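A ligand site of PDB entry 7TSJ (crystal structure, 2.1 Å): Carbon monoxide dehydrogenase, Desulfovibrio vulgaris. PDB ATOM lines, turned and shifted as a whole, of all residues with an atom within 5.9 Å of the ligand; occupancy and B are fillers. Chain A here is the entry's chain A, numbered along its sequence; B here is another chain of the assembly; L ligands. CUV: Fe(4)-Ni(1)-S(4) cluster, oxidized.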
ATOM      1  N   HIS A 105     -19.688  11.940 -21.855  1.00  0.00           N
ATOM      2  CA  HIS A 105     -20.114  10.980 -22.867  1.00  0.00           C
ATOM      3  C   HIS A 105     -21.379  11.412 -23.581  1.00  0.00           C
ATOM      4  O   HIS A 105     -21.508  11.181 -24.786  1.00  0.00           O
ATOM      5  CB  HIS A 105     -20.306   9.598 -22.223  1.00  0.00           C
ATOM      6  CG  HIS A 105     -19.014   8.965 -21.828  1.00  0.00           C
ATOM      7  ND1 HIS A 105     -18.851   8.264 -20.645  1.00  0.00           N
ATOM      8  CD2 HIS A 105     -17.810   8.953 -22.443  1.00  0.00           C
ATOM      9  CE1 HIS A 105     -17.606   7.836 -20.564  1.00  0.00           C
ATOM     10  NE2 HIS A 105     -16.951   8.249 -21.638  1.00  0.00           N
ATOM     11  N   GLY A 273      -8.155  13.668 -28.124  1.00  0.00           N
ATOM     12  CA  GLY A 273      -9.549  13.823 -27.770  1.00  0.00           C
ATOM     13  C   GLY A 273     -10.419  12.627 -28.096  1.00  0.00           C
ATOM     14  O   GLY A 273     -10.019  11.475 -27.898  1.00  0.00           O
ATOM     15  N   HIS A 274     -11.632  12.888 -28.620  1.00  0.00           N
ATOM     16  CA  HIS A 274     -12.655  11.853 -28.652  1.00  0.00           C
ATOM     17  C   HIS A 274     -13.501  11.794 -29.924  1.00  0.00           C
ATOM     18  O   HIS A 274     -14.307  10.869 -30.052  1.00  0.00           O
ATOM     19  CB  HIS A 274     -13.617  12.030 -27.449  1.00  0.00           C
ATOM     20  CG  HIS A 274     -13.051  11.545 -26.157  1.00  0.00           C
ATOM     21  ND1 HIS A 274     -12.070  12.224 -25.461  1.00  0.00           N
ATOM     22  CD2 HIS A 274     -13.314  10.418 -25.434  1.00  0.00           C
ATOM     23  CE1 HIS A 274     -11.748  11.542 -24.381  1.00  0.00           C
ATOM     24  NE2 HIS A 274     -12.483  10.444 -24.338  1.00  0.00           N
ATOM     25  N   LEU A 308      -3.981   9.526 -30.497  1.00  0.00           N
ATOM     26  CA  LEU A 308      -3.871   9.670 -29.053  1.00  0.00           C
ATOM     27  C   LEU A 308      -5.243   9.510 -28.418  1.00  0.00           C
ATOM     28  O   LEU A 308      -6.261   9.823 -29.031  1.00  0.00           O
ATOM     29  CB  LEU A 308      -3.288  11.035 -28.659  1.00  0.00           C
ATOM     30  CG  LEU A 308      -1.851  11.385 -29.063  1.00  0.00           C
ATOM     31  CD1 LEU A 308      -1.584  12.881 -28.846  1.00  0.00           C
ATOM     32  CD2 LEU A 308      -0.866  10.551 -28.265  1.00  0.00           C
ATOM     33  N   CYS A 309      -5.259   9.002 -27.192  1.00  0.00           N
ATOM     34  CA  CYS A 309      -6.472   8.928 -26.378  1.00  0.00           C
ATOM     35  C   CYS A 309      -7.580   8.175 -27.117  1.00  0.00           C
ATOM     36  O   CYS A 309      -7.322   7.171 -27.792  1.00  0.00           O
ATOM     37  CB  CYS A 309      -6.916  10.346 -25.974  1.00  0.00           C
ATOM     38  SG  CYS A 309      -8.149  10.460 -24.606  1.00  0.00           S
ATOM     39  N   CYS A 310      -8.807   8.670 -27.033  1.00  0.00           N
ATOM     40  CA  CYS A 310      -9.946   7.891 -27.480  1.00  0.00           C
ATOM     41  C   CYS A 310     -10.201   8.038 -28.979  1.00  0.00           C
ATOM     42  O   CYS A 310     -10.545   7.059 -29.655  1.00  0.00           O
ATOM     43  CB  CYS A 310     -11.194   8.254 -26.666  1.00  0.00           C
ATOM     44  SG  CYS A 310     -11.290   7.288 -25.125  1.00  0.00           S
ATOM     45  N   ASN A 313      -7.859   5.587 -30.272  1.00  0.00           N
ATOM     46  CA  ASN A 313      -8.466   4.257 -30.157  1.00  0.00           C
ATOM     47  C   ASN A 313      -9.439   4.006 -31.302  1.00  0.00           C
ATOM     48  O   ASN A 313      -9.372   2.964 -31.967  1.00  0.00           O
ATOM     49  CB  ASN A 313      -9.187   4.106 -28.812  1.00  0.00           C
ATOM     50  CG  ASN A 313      -8.257   3.675 -27.689  1.00  0.00           C
ATOM     51  OD1 ASN A 313      -7.870   2.507 -27.616  1.00  0.00           O
ATOM     52  ND2 ASN A 313      -7.912   4.602 -26.789  1.00  0.00           N
ATOM     53  N   MET A 323      -1.267   4.109 -33.097  1.00  0.00           N
ATOM     54  CA  MET A 323      -1.529   4.868 -31.878  1.00  0.00           C
ATOM     55  C   MET A 323      -0.215   5.254 -31.196  1.00  0.00           C
ATOM     56  O   MET A 323       0.573   4.367 -30.816  1.00  0.00           O
ATOM     57  CB  MET A 323      -2.405   4.042 -30.944  1.00  0.00           C
ATOM     58  CG  MET A 323      -2.801   4.765 -29.685  1.00  0.00           C
ATOM     59  SD  MET A 323      -4.520   4.463 -29.287  1.00  0.00           S
ATOM     60  CE  MET A 323      -4.659   5.460 -27.792  1.00  0.00           C
ATOM     61  N   ASN A 326      -1.022   6.664 -24.823  1.00  0.00           N
ATOM     62  CA  ASN A 326      -2.188   6.906 -23.989  1.00  0.00           C
ATOM     63  C   ASN A 326      -1.973   8.181 -23.158  1.00  0.00           C
ATOM     64  O   ASN A 326      -1.138   9.033 -23.508  1.00  0.00           O
ATOM     65  CB  ASN A 326      -2.475   5.650 -23.141  1.00  0.00           C
ATOM     66  CG  ASN A 326      -1.220   5.064 -22.480  1.00  0.00           C
ATOM     67  OD1 ASN A 326      -0.195   5.737 -22.378  1.00  0.00           O
ATOM     68  ND2 ASN A 326      -1.310   3.818 -22.025  1.00  0.00           N
ATOM     69  N   HIS A 327      -2.677   8.293 -22.035  1.00  0.00           N
ATOM     70  CA  HIS A 327      -2.893   9.605 -21.417  1.00  0.00           C
ATOM     71  C   HIS A 327      -1.607  10.252 -20.911  1.00  0.00           C
ATOM     72  O   HIS A 327      -1.329  11.420 -21.219  1.00  0.00           O
ATOM     73  CB  HIS A 327      -3.907   9.466 -20.271  1.00  0.00           C
ATOM     74  CG  HIS A 327      -4.029  10.703 -19.430  1.00  0.00           C
ATOM     75  ND1 HIS A 327      -4.089  10.665 -18.061  1.00  0.00           N
ATOM     76  CD2 HIS A 327      -4.077  12.011 -19.781  1.00  0.00           C
ATOM     77  CE1 HIS A 327      -4.174  11.893 -17.593  1.00  0.00           C
ATOM     78  NE2 HIS A 327      -4.171  12.733 -18.617  1.00  0.00           N
ATOM     79  N   GLN A 347     -12.111  16.511 -24.197  1.00  0.00           N
ATOM     80  CA  GLN A 347     -12.055  15.541 -23.114  1.00  0.00           C
ATOM     81  C   GLN A 347     -10.675  14.899 -22.986  1.00  0.00           C
ATOM     82  O   GLN A 347     -10.130  14.338 -23.961  1.00  0.00           O
ATOM     83  CB  GLN A 347     -13.135  14.453 -23.262  1.00  0.00           C
ATOM     84  CG  GLN A 347     -14.593  14.947 -23.195  1.00  0.00           C
ATOM     85  CD  GLN A 347     -14.954  15.559 -21.845  1.00  0.00           C
ATOM     86  OE1 GLN A 347     -14.341  15.249 -20.824  1.00  0.00           O
ATOM     87  NE2 GLN A 347     -15.976  16.440 -21.840  1.00  0.00           N
ATOM     88  N   CYS A 348     -10.113  14.976 -21.768  1.00  0.00           N
ATOM     89  CA  CYS A 348      -8.829  14.369 -21.385  1.00  0.00           C
ATOM     90  C   CYS A 348      -7.645  14.987 -22.132  1.00  0.00           C
ATOM     91  O   CYS A 348      -6.558  14.401 -22.157  1.00  0.00           O
ATOM     92  CB  CYS A 348      -8.852  12.841 -21.578  1.00  0.00           C
ATOM     93  SG  CYS A 348     -10.168  11.980 -20.660  1.00  0.00           S
ATOM     94  N   VAL A 454     -10.326  -1.331 -18.373  1.00  0.00           N
ATOM     95  CA  VAL A 454     -10.605  -0.056 -18.986  1.00  0.00           C
ATOM     96  C   VAL A 454      -9.934   1.030 -18.144  1.00  0.00           C
ATOM     97  O   VAL A 454      -9.253   0.751 -17.169  1.00  0.00           O
ATOM     98  CB  VAL A 454     -12.121   0.183 -19.113  1.00  0.00           C
ATOM     99  CG1 VAL A 454     -12.790  -1.126 -19.564  1.00  0.00           C
ATOM    100  CG2 VAL A 454     -12.696   0.621 -17.782  1.00  0.00           C
ATOM    101  N   GLY A 455     -10.105   2.272 -18.544  1.00  0.00           N
ATOM    102  CA  GLY A 455      -9.578   3.345 -17.728  1.00  0.00           C
ATOM    103  C   GLY A 455      -8.161   3.765 -18.058  1.00  0.00           C
ATOM    104  O   GLY A 455      -7.431   3.152 -18.862  1.00  0.00           O
ATOM    105  N   CYS A 456      -7.746   4.816 -17.369  1.00  0.00           N
ATOM    106  CA  CYS A 456      -6.752   5.754 -17.851  1.00  0.00           C
ATOM    107  C   CYS A 456      -5.349   5.373 -17.369  1.00  0.00           C
ATOM    108  O   CYS A 456      -5.057   4.197 -17.118  1.00  0.00           O
ATOM    109  CB  CYS A 456      -7.198   7.155 -17.385  1.00  0.00           C
ATOM    110  SG  CYS A 456      -8.983   7.264 -16.808  1.00  0.00           S
ATOM    111  N   ASN A 457      -4.446   6.352 -17.292  1.00  0.00           N
ATOM    112  CA  ASN A 457      -3.277   6.366 -16.436  1.00  0.00           C
ATOM    113  C   ASN A 457      -3.500   7.393 -15.334  1.00  0.00           C
ATOM    114  O   ASN A 457      -4.332   8.289 -15.461  1.00  0.00           O
ATOM    115  CB  ASN A 457      -1.999   6.737 -17.187  1.00  0.00           C
ATOM    116  CG  ASN A 457      -1.673   5.802 -18.326  1.00  0.00           C
ATOM    117  OD1 ASN A 457      -1.307   6.247 -19.411  1.00  0.00           O
ATOM    118  ND2 ASN A 457      -1.771   4.493 -18.088  1.00  0.00           N
ATOM    119  N   THR A 484     -10.043  -1.527 -23.439  1.00  0.00           N
ATOM    120  CA  THR A 484     -10.487  -0.255 -24.019  1.00  0.00           C
ATOM    121  C   THR A 484      -9.677   0.882 -23.408  1.00  0.00           C
ATOM    122  O   THR A 484      -8.994   0.733 -22.395  1.00  0.00           O
ATOM    123  CB  THR A 484     -11.976   0.003 -23.779  1.00  0.00           C
ATOM    124  OG1 THR A 484     -12.195   0.178 -22.378  1.00  0.00           O
ATOM    125  CG2 THR A 484     -12.837  -1.158 -24.307  1.00  0.00           C
ATOM    126  N   GLY A 485      -9.732   2.039 -24.069  1.00  0.00           N
ATOM    127  CA  GLY A 485      -9.160   3.247 -23.471  1.00  0.00           C
ATOM    128  C   GLY A 485      -7.642   3.199 -23.406  1.00  0.00           C
ATOM    129  O   GLY A 485      -6.976   2.731 -24.337  1.00  0.00           O
ATOM    130  N   CYS A 486      -7.090   3.702 -22.295  1.00  0.00           N
ATOM    131  CA  CYS A 486      -5.630   3.739 -22.137  1.00  0.00           C
ATOM    132  C   CYS A 486      -5.014   2.347 -22.021  1.00  0.00           C
ATOM    133  O   CYS A 486      -3.837   2.165 -22.343  1.00  0.00           O
ATOM    134  CB  CYS A 486      -5.262   4.570 -20.911  1.00  0.00           C
ATOM    135  SG  CYS A 486      -5.437   6.379 -21.088  1.00  0.00           S
ATOM    136  N   VAL A 487      -5.779   1.364 -21.539  1.00  0.00           N
ATOM    137  CA  VAL A 487      -5.241   0.010 -21.427  1.00  0.00           C
ATOM    138  C   VAL A 487      -4.819  -0.514 -22.786  1.00  0.00           C
ATOM    139  O   VAL A 487      -3.914  -1.349 -22.900  1.00  0.00           O
ATOM    140  CB  VAL A 487      -6.269  -0.914 -20.745  1.00  0.00           C
ATOM    141  CG1 VAL A 487      -5.643  -2.271 -20.406  1.00  0.00           C
ATOM    142  CG2 VAL A 487      -6.841  -0.233 -19.503  1.00  0.00           C
ATOM    143  N   SER A 526     -12.471   2.695 -27.719  1.00  0.00           N
ATOM    144  CA  SER A 526     -12.280   3.849 -26.835  1.00  0.00           C
ATOM    145  C   SER A 526     -13.100   3.700 -25.565  1.00  0.00           C
ATOM    146  O   SER A 526     -13.812   2.699 -25.355  1.00  0.00           O
ATOM    147  CB  SER A 526     -12.687   5.134 -27.554  1.00  0.00           C
ATOM    148  OG  SER A 526     -14.067   5.120 -27.836  1.00  0.00           O
ATOM    149  N   CYS A 527     -13.026   4.714 -24.705  1.00  0.00           N
ATOM    150  CA  CYS A 527     -13.791   4.677 -23.473  1.00  0.00           C
ATOM    151  C   CYS A 527     -15.298   4.673 -23.747  1.00  0.00           C
ATOM    152  O   CYS A 527     -16.057   4.093 -22.957  1.00  0.00           O
ATOM    153  CB  CYS A 527     -13.417   5.851 -22.574  1.00  0.00           C
ATOM    154  SG  CYS A 527     -14.169   7.436 -23.086  1.00  0.00           S
ATOM    155  N   VAL A 528     -15.734   5.249 -24.861  1.00  0.00           N
ATOM    156  CA  VAL A 528     -17.158   5.214 -25.167  1.00  0.00           C
ATOM    157  C   VAL A 528     -17.575   3.810 -25.587  1.00  0.00           C
ATOM    158  O   VAL A 528     -18.687   3.364 -25.292  1.00  0.00           O
ATOM    159  CB  VAL A 528     -17.524   6.270 -26.238  1.00  0.00           C
ATOM    160  CG1 VAL A 528     -16.743   7.579 -25.979  1.00  0.00           C
ATOM    161  CG2 VAL A 528     -17.255   5.760 -27.636  1.00  0.00           C
ATOM    162  N   TYR A 561      -8.343   8.008 -13.648  1.00  0.00           N
ATOM    163  CA  TYR A 561      -8.284   9.353 -13.093  1.00  0.00           C
ATOM    164  C   TYR A 561      -9.550  10.177 -13.319  1.00  0.00           C
ATOM    165  O   TYR A 561      -9.830  11.061 -12.508  1.00  0.00           O
ATOM    166  CB  TYR A 561      -7.058  10.138 -13.651  1.00  0.00           C
ATOM    167  CG  TYR A 561      -7.380  10.880 -14.915  1.00  0.00           C
ATOM    168  CD1 TYR A 561      -7.955  12.155 -14.859  1.00  0.00           C
ATOM    169  CD2 TYR A 561      -7.168  10.308 -16.159  1.00  0.00           C
ATOM    170  CE1 TYR A 561      -8.311  12.830 -16.005  1.00  0.00           C
ATOM    171  CE2 TYR A 561      -7.511  10.993 -17.334  1.00  0.00           C
ATOM    172  CZ  TYR A 561      -8.096  12.254 -17.235  1.00  0.00           C
ATOM    173  OH  TYR A 561      -8.466  12.971 -18.349  1.00  0.00           O
ATOM    174  N   SER A 562     -10.323   9.939 -14.378  1.00  0.00           N
ATOM    175  CA  SER A 562     -11.317  10.909 -14.832  1.00  0.00           C
ATOM    176  C   SER A 562     -12.705  10.609 -14.289  1.00  0.00           C
ATOM    177  O   SER A 562     -13.017   9.499 -13.848  1.00  0.00           O
ATOM    178  CB  SER A 562     -11.380  10.932 -16.360  1.00  0.00           C
ATOM    179  OG  SER A 562     -11.772   9.658 -16.821  1.00  0.00           O
ATOM    180  N   LYS A 564     -15.202  10.541 -16.360  1.00  0.00           N
ATOM    181  CA  LYS A 564     -15.688   9.567 -17.352  1.00  0.00           C
ATOM    182  C   LYS A 564     -15.437   8.128 -16.913  1.00  0.00           C
ATOM    183  O   LYS A 564     -16.296   7.259 -17.073  1.00  0.00           O
ATOM    184  CB  LYS A 564     -15.025   9.841 -18.712  1.00  0.00           C
ATOM    185  CG  LYS A 564     -15.717  10.917 -19.541  1.00  0.00           C
ATOM    186  CD  LYS A 564     -14.741  11.794 -20.345  1.00  0.00           C
ATOM    187  CE  LYS A 564     -13.803  10.989 -21.234  1.00  0.00           C
ATOM    188  NZ  LYS A 564     -14.557  10.367 -22.348  1.00  0.00           N
ATOM    189  N   ALA A 565     -14.257   7.851 -16.352  1.00  0.00           N
ATOM    190  CA  ALA A 565     -13.974   6.470 -15.958  1.00  0.00           C
ATOM    191  C   ALA A 565     -14.827   6.068 -14.764  1.00  0.00           C
ATOM    192  O   ALA A 565     -15.291   4.921 -14.676  1.00  0.00           O
ATOM    193  CB  ALA A 565     -12.479   6.301 -15.644  1.00  0.00           C
ATOM    194  N   ILE A 568     -18.159   5.118 -16.025  1.00  0.00           N
ATOM    195  CA  ILE A 568     -18.084   3.766 -16.581  1.00  0.00           C
ATOM    196  C   ILE A 568     -18.087   2.740 -15.471  1.00  0.00           C
ATOM    197  O   ILE A 568     -18.866   1.777 -15.502  1.00  0.00           O
ATOM    198  CB  ILE A 568     -16.832   3.618 -17.479  1.00  0.00           C
ATOM    199  CG1 ILE A 568     -17.036   4.346 -18.813  1.00  0.00           C
ATOM    200  CG2 ILE A 568     -16.517   2.123 -17.753  1.00  0.00           C
ATOM    201  CD1 ILE A 568     -15.738   4.772 -19.425  1.00  0.00           C
ATOM    202  N   HIS B 210     -15.491  18.994 -17.221  1.00  0.00           N
ATOM    203  CA  HIS B 210     -14.642  17.814 -17.113  1.00  0.00           C
ATOM    204  C   HIS B 210     -13.209  18.204 -17.495  1.00  0.00           C
ATOM    205  O   HIS B 210     -12.977  19.111 -18.305  1.00  0.00           O
ATOM    206  CB  HIS B 210     -15.176  16.687 -18.023  1.00  0.00           C
ATOM    207  CG  HIS B 210     -14.494  15.354 -17.844  1.00  0.00           C
ATOM    208  ND1 HIS B 210     -13.189  15.118 -18.220  1.00  0.00           N
ATOM    209  CD2 HIS B 210     -14.963  14.169 -17.374  1.00  0.00           C
ATOM    210  CE1 HIS B 210     -12.868  13.861 -17.948  1.00  0.00           C
ATOM    211  NE2 HIS B 210     -13.931  13.256 -17.437  1.00  0.00           N
HETATM  212 NI   CUV L   1     -12.061   8.941 -23.131  1.00  0.00          NI
HETATM  213  S1  CUV L   1      -9.388   5.278 -20.566  1.00  0.00           S
HETATM  214  S2  CUV L   1      -7.500   9.216 -20.243  1.00  0.00           S
HETATM  215  S3  CUV L   1      -7.624   6.614 -24.027  1.00  0.00           S
HETATM  216  S4  CUV L   1     -11.701   8.334 -19.361  1.00  0.00           S
HETATM  217 FE1  CUV L   1     -10.019   9.601 -21.028  1.00  0.00          FE
HETATM  218 FE2  CUV L   1      -9.332   8.606 -23.650  1.00  0.00          FE
HETATM  219 FE3  CUV L   1      -9.258   7.446 -19.089  1.00  0.00          FE
HETATM  220 FE4  CUV L   1      -7.666   6.956 -21.466  1.00  0.00          FE
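CB of His 327 touches S2 of the ligand (3.6 Å).
Gly 485 touches the ligand.
Tyr 561 touches the ligand.
Lys 564 touches the ligand.
Ala 565 touches the ligand.
15 residues have an atom within 4 Å of the ligand: His 274, Cys 309, Cys 310, Asn 313, His 327, Cys 348, Gly 455, Cys 456, Gly 485, Cys 486, Cys 527, Tyr 561, Ser 562, Lys 564 and Ala 565.
NZ of Lys 564 sits close to NE2 of His 274 (2.9 Å).
The side-chain sulfur of Cys 456 lies close to the side-chain hydroxyl of Ser 562, at 3.7 Å.
The backbone carbonyl oxygen (O) of Gly 455 lies close to the backbone NH (N) of Cys 486, at 3.5 Å.
SG of Cys 486 lies close to N of His 327 (3.5 Å).
O of Cys 309 sits at hydrogen-bond distance from ND2 of Asn 313, 2.8 Å away.
The side-chain sulfur (SG) of Cys 348 sits close to the side-chain hydroxyl (OH) of Tyr 561 (3.0 Å).
SG of Cys 527 sits close to NZ of Lys 564, 3.0 Å away.
The backbone NH (N) of Asn 313 lies within hydrogen-bond range of the side-chain sulfur (SD) of Met 323 (3.7 Å).
NI of the ligand is bound by NE2 of His 274 (2.0 Å).
The backbone NH (N) of Cys 456 lies close to a sulfur (S1) of the ligand (3.6 Å).
The side-chain sulfur (SG) of Cys 456 is bound to an iron atom (FE3) of the ligand, 2.3 Å away.
N of Cys 486 lies close to S1 of the ligand, at 3.3 Å.
The side-chain sulfur (SG) of Cys 486 binds an iron atom (FE4) of the ligand.
FE2 of the ligand is bound by SG of Cys 309 (2.4 Å).
The side-chain sulfur (SG) of Cys 348 binds an iron atom (FE1) of the ligand.
NI of the ligand is bound by SG of Cys 527 (2.6 Å).
SG of Cys 310 binds NI of the ligand, at 2.7 Å.
The side-chain hydroxyl of Ser 562 lies close to a sulfur (S4) of the ligand (2.9 Å).
N of Gly 455 sits close to S1 of the ligand (3.7 Å).
The side-chain amide nitrogen of Asn 313 lies close to a sulfur (S3) of the ligand (3.4 Å).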
